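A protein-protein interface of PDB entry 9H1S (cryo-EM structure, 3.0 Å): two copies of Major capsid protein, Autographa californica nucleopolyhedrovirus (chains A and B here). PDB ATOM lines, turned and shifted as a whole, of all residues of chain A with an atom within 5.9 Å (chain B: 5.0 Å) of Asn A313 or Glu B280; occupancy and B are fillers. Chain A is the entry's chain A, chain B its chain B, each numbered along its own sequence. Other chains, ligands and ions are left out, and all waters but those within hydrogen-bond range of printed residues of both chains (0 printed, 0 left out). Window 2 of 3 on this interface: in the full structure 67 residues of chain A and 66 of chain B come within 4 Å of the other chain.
The side-chain carboxylate of Glu B280 is in salt-bridge range of the guanidinium group of Arg B283, at 2.7 Å.
OD2 of Asp B277 is in salt-bridge range of NH2 of Arg B279.
O of Glu B280 sits at hydrogen-bond distance from OG1 of Thr B284, at 2.7 Å.
Of the 8 printed residues of chain B, 5 touch a printed residue of chain A.
Hydrophobic or aromatic side chains of chain B within 4 Å of the printed part of chain A: Leu B281.
Of the 7 printed residues of chain A, 4 touch a printed residue of chain B.
Among the printed residues, 6 pairs touch across the chains.
No position is printed for both chains.
Printed residues of chain B within 4 Å of Asp A43: Thr B284 (3.95 Å).
Of the printed residues of chain B, Asp A44 touches Thr B284.
Arg A312 touches none of the printed residues of chain B.
Of chain B, only Glu B280 comes within 4 Å of Asn A313.
Of the printed residues of chain A, Thr B278 touches Leu A311.
Glu B280 touches one residue of chain A.
Arg B283 touches none of the printed residues of chain A.
The nearest printed residue of chain A that does not touch Leu B281 is Arg A312 (4.03 Å).
Among the printed residues, pairs that only touch across the chains: Leu A311 with Leu B281 (3.5 Å), Leu A311 with Thr B278 (3.7 Å), Leu A311 with Asp B277 (3.8 Å), Asp A44 with Thr B284 (3.9 Å) and Asp A43 with Thr B284 (3.95 Å).
OE2 of Glu B280 is in hydrogen-bond range of ND2 of Asn A313, at 2.9 Å.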
ATOM      1  N   ASP A  43     -10.059 -21.090   3.008  1.00  0.00           N
ATOM      2  CA  ASP A  43      -8.736 -21.651   2.913  1.00  0.00           C
ATOM      3  C   ASP A  43      -8.130 -21.785   4.286  1.00  0.00           C
ATOM      4  O   ASP A  43      -7.460 -20.876   4.772  1.00  0.00           O
ATOM      5  CB  ASP A  43      -7.845 -20.797   2.025  1.00  0.00           C
ATOM      6  CG  ASP A  43      -6.484 -21.430   1.777  1.00  0.00           C
ATOM      7  OD1 ASP A  43      -6.193 -22.429   2.392  1.00  0.00           O
ATOM      8  OD2 ASP A  43      -5.755 -20.921   0.961  1.00  0.00           O
ATOM      9  N   ASP A  44      -8.348 -22.933   4.898  1.00  0.00           N
ATOM     10  CA  ASP A  44      -7.809 -23.180   6.217  1.00  0.00           C
ATOM     11  C   ASP A  44      -7.384 -24.629   6.357  1.00  0.00           C
ATOM     12  O   ASP A  44      -7.299 -25.354   5.368  1.00  0.00           O
ATOM     13  CB  ASP A  44      -8.832 -22.767   7.278  1.00  0.00           C
ATOM     14  CG  ASP A  44     -10.132 -23.544   7.233  1.00  0.00           C
ATOM     15  OD1 ASP A  44     -10.111 -24.689   6.856  1.00  0.00           O
ATOM     16  OD2 ASP A  44     -11.140 -22.978   7.593  1.00  0.00           O
ATOM     17  N   LEU A 311       1.376 -17.644  13.356  1.00  0.00           N
ATOM     18  CA  LEU A 311       0.220 -16.914  12.914  1.00  0.00           C
ATOM     19  C   LEU A 311       0.053 -16.937  11.402  1.00  0.00           C
ATOM     20  O   LEU A 311      -0.887 -16.338  10.878  1.00  0.00           O
ATOM     21  CB  LEU A 311       0.342 -15.496  13.413  1.00  0.00           C
ATOM     22  CG  LEU A 311       0.446 -15.371  14.932  1.00  0.00           C
ATOM     23  CD1 LEU A 311       0.682 -13.922  15.290  1.00  0.00           C
ATOM     24  CD2 LEU A 311      -0.810 -15.915  15.576  1.00  0.00           C
ATOM     25  N   ARG A 312       0.965 -17.617  10.700  1.00  0.00           N
ATOM     26  CA  ARG A 312       0.873 -17.783   9.260  1.00  0.00           C
ATOM     27  C   ARG A 312      -0.499 -18.296   8.864  1.00  0.00           C
ATOM     28  O   ARG A 312      -1.054 -19.185   9.512  1.00  0.00           O
ATOM     29  CB  ARG A 312       1.929 -18.758   8.803  1.00  0.00           C
ATOM     30  CG  ARG A 312       1.737 -20.155   9.372  1.00  0.00           C
ATOM     31  CD  ARG A 312       2.971 -20.967   9.260  1.00  0.00           C
ATOM     32  NE  ARG A 312       3.274 -21.295   7.889  1.00  0.00           N
ATOM     33  CZ  ARG A 312       4.470 -21.710   7.435  1.00  0.00           C
ATOM     34  NH1 ARG A 312       5.500 -21.826   8.250  1.00  0.00           N
ATOM     35  NH2 ARG A 312       4.602 -21.994   6.153  1.00  0.00           N
ATOM     36  N   ASN A 313      -1.039 -17.755   7.780  1.00  0.00           N
ATOM     37  CA  ASN A 313      -2.375 -18.129   7.344  1.00  0.00           C
ATOM     38  C   ASN A 313      -2.414 -19.212   6.285  1.00  0.00           C
ATOM     39  O   ASN A 313      -3.476 -19.495   5.733  1.00  0.00           O
ATOM     40  CB  ASN A 313      -3.083 -16.923   6.813  1.00  0.00           C
ATOM     41  CG  ASN A 313      -2.424 -16.428   5.561  1.00  0.00           C
ATOM     42  OD1 ASN A 313      -1.296 -16.834   5.259  1.00  0.00           O
ATOM     43  ND2 ASN A 313      -3.088 -15.574   4.825  1.00  0.00           N
ATOM     44  N   ASP A 314      -1.281 -19.818   5.986  1.00  0.00           N
ATOM     45  CA  ASP A 314      -1.278 -20.877   5.003  1.00  0.00           C
ATOM     46  C   ASP A 314      -1.428 -22.216   5.684  1.00  0.00           C
ATOM     47  O   ASP A 314      -1.567 -22.291   6.905  1.00  0.00           O
ATOM     48  CB  ASP A 314       0.004 -20.850   4.183  1.00  0.00           C
ATOM     49  CG  ASP A 314       1.229 -21.168   5.019  1.00  0.00           C
ATOM     50  OD1 ASP A 314       1.068 -21.517   6.163  1.00  0.00           O
ATOM     51  OD2 ASP A 314       2.322 -21.083   4.512  1.00  0.00           O
ATOM     52  N   PHE A 315      -1.369 -23.275   4.902  1.00  0.00           N
ATOM     53  CA  PHE A 315      -1.433 -24.603   5.460  1.00  0.00           C
ATOM     54  C   PHE A 315      -0.118 -25.312   5.323  1.00  0.00           C
ATOM     55  O   PHE A 315       0.522 -25.274   4.272  1.00  0.00           O
ATOM     56  CB  PHE A 315      -2.510 -25.452   4.814  1.00  0.00           C
ATOM     57  CG  PHE A 315      -2.414 -26.855   5.319  1.00  0.00           C
ATOM     58  CD1 PHE A 315      -2.842 -27.185   6.591  1.00  0.00           C
ATOM     59  CD2 PHE A 315      -1.856 -27.842   4.531  1.00  0.00           C
ATOM     60  CE1 PHE A 315      -2.709 -28.475   7.063  1.00  0.00           C
ATOM     61  CE2 PHE A 315      -1.726 -29.127   5.001  1.00  0.00           C
ATOM     62  CZ  PHE A 315      -2.149 -29.447   6.269  1.00  0.00           C
ATOM     63  N   ASP B 277       0.733 -10.260  14.310  1.00  0.00           N
ATOM     64  CA  ASP B 277      -0.516  -9.809  13.720  1.00  0.00           C
ATOM     65  C   ASP B 277      -1.462 -10.980  13.566  1.00  0.00           C
ATOM     66  O   ASP B 277      -1.296 -11.815  12.679  1.00  0.00           O
ATOM     67  CB  ASP B 277      -0.270  -9.149  12.374  1.00  0.00           C
ATOM     68  CG  ASP B 277      -1.523  -8.535  11.769  1.00  0.00           C
ATOM     69  OD1 ASP B 277      -2.609  -8.783  12.245  1.00  0.00           O
ATOM     70  OD2 ASP B 277      -1.377  -7.790  10.829  1.00  0.00           O
ATOM     71  N   THR B 278      -2.449 -11.044  14.442  1.00  0.00           N
ATOM     72  CA  THR B 278      -3.381 -12.153  14.468  1.00  0.00           C
ATOM     73  C   THR B 278      -4.664 -11.882  13.691  1.00  0.00           C
ATOM     74  O   THR B 278      -5.565 -12.723  13.675  1.00  0.00           O
ATOM     75  CB  THR B 278      -3.759 -12.477  15.914  1.00  0.00           C
ATOM     76  OG1 THR B 278      -4.473 -11.373  16.481  1.00  0.00           O
ATOM     77  CG2 THR B 278      -2.502 -12.689  16.732  1.00  0.00           C
ATOM     78  N   ARG B 279      -4.756 -10.713  13.054  1.00  0.00           N
ATOM     79  CA  ARG B 279      -5.992 -10.337  12.384  1.00  0.00           C
ATOM     80  C   ARG B 279      -6.279 -11.182  11.171  1.00  0.00           C
ATOM     81  O   ARG B 279      -7.432 -11.335  10.776  1.00  0.00           O
ATOM     82  CB  ARG B 279      -5.926  -8.906  11.933  1.00  0.00           C
ATOM     83  CG  ARG B 279      -5.878  -7.882  13.037  1.00  0.00           C
ATOM     84  CD  ARG B 279      -5.717  -6.538  12.456  1.00  0.00           C
ATOM     85  NE  ARG B 279      -4.458  -6.452  11.747  1.00  0.00           N
ATOM     86  CZ  ARG B 279      -4.068  -5.419  10.979  1.00  0.00           C
ATOM     87  NH1 ARG B 279      -4.847  -4.367  10.836  1.00  0.00           N
ATOM     88  NH2 ARG B 279      -2.899  -5.471  10.370  1.00  0.00           N
ATOM     89  N   GLU B 280      -5.240 -11.752  10.592  1.00  0.00           N
ATOM     90  CA  GLU B 280      -5.411 -12.602   9.446  1.00  0.00           C
ATOM     91  C   GLU B 280      -6.077 -13.897   9.835  1.00  0.00           C
ATOM     92  O   GLU B 280      -6.896 -14.422   9.082  1.00  0.00           O
ATOM     93  CB  GLU B 280      -4.086 -12.852   8.777  1.00  0.00           C
ATOM     94  CG  GLU B 280      -4.194 -13.708   7.546  1.00  0.00           C
ATOM     95  CD  GLU B 280      -5.055 -13.128   6.460  1.00  0.00           C
ATOM     96  OE1 GLU B 280      -5.399 -11.972   6.521  1.00  0.00           O
ATOM     97  OE2 GLU B 280      -5.342 -13.855   5.536  1.00  0.00           O
ATOM     98  N   LEU B 281      -5.730 -14.413  11.010  1.00  0.00           N
ATOM     99  CA  LEU B 281      -6.356 -15.626  11.486  1.00  0.00           C
ATOM    100  C   LEU B 281      -7.795 -15.351  11.830  1.00  0.00           C
ATOM    101  O   LEU B 281      -8.660 -16.195  11.601  1.00  0.00           O
ATOM    102  CB  LEU B 281      -5.656 -16.161  12.719  1.00  0.00           C
ATOM    103  CG  LEU B 281      -4.244 -16.678  12.508  1.00  0.00           C
ATOM    104  CD1 LEU B 281      -3.681 -17.089  13.855  1.00  0.00           C
ATOM    105  CD2 LEU B 281      -4.267 -17.838  11.530  1.00  0.00           C
ATOM    106  N   ASP B 282      -8.059 -14.159  12.357  1.00  0.00           N
ATOM    107  CA  ASP B 282      -9.422 -13.781  12.670  1.00  0.00           C
ATOM    108  C   ASP B 282     -10.267 -13.762  11.420  1.00  0.00           C
ATOM    109  O   ASP B 282     -11.396 -14.250  11.425  1.00  0.00           O
ATOM    110  CB  ASP B 282      -9.466 -12.424  13.346  1.00  0.00           C
ATOM    111  CG  ASP B 282      -8.940 -12.481  14.761  1.00  0.00           C
ATOM    112  OD1 ASP B 282      -8.761 -13.565  15.262  1.00  0.00           O
ATOM    113  OD2 ASP B 282      -8.749 -11.442  15.345  1.00  0.00           O
ATOM    114  N   ARG B 283      -9.709 -13.225  10.341  1.00  0.00           N
ATOM    115  CA  ARG B 283     -10.385 -13.216   9.059  1.00  0.00           C
ATOM    116  C   ARG B 283     -10.579 -14.625   8.540  1.00  0.00           C
ATOM    117  O   ARG B 283     -11.671 -14.987   8.097  1.00  0.00           O
ATOM    118  CB  ARG B 283      -9.586 -12.393   8.073  1.00  0.00           C
ATOM    119  CG  ARG B 283      -9.677 -10.899   8.303  1.00  0.00           C
ATOM    120  CD  ARG B 283      -9.071 -10.134   7.190  1.00  0.00           C
ATOM    121  NE  ARG B 283      -7.620 -10.241   7.199  1.00  0.00           N
ATOM    122  CZ  ARG B 283      -6.807  -9.408   7.876  1.00  0.00           C
ATOM    123  NH1 ARG B 283      -7.307  -8.413   8.575  1.00  0.00           N
ATOM    124  NH2 ARG B 283      -5.503  -9.597   7.830  1.00  0.00           N
ATOM    125  N   THR B 284      -9.539 -15.439   8.662  1.00  0.00           N
ATOM    126  CA  THR B 284      -9.570 -16.822   8.227  1.00  0.00           C
ATOM    127  C   THR B 284     -10.691 -17.605   8.880  1.00  0.00           C
ATOM    128  O   THR B 284     -11.387 -18.377   8.220  1.00  0.00           O
ATOM    129  CB  THR B 284      -8.239 -17.510   8.546  1.00  0.00           C
ATOM    130  OG1 THR B 284      -7.180 -16.846   7.846  1.00  0.00           O
ATOM    131  CG2 THR B 284      -8.286 -18.969   8.136  1.00  0.00           C
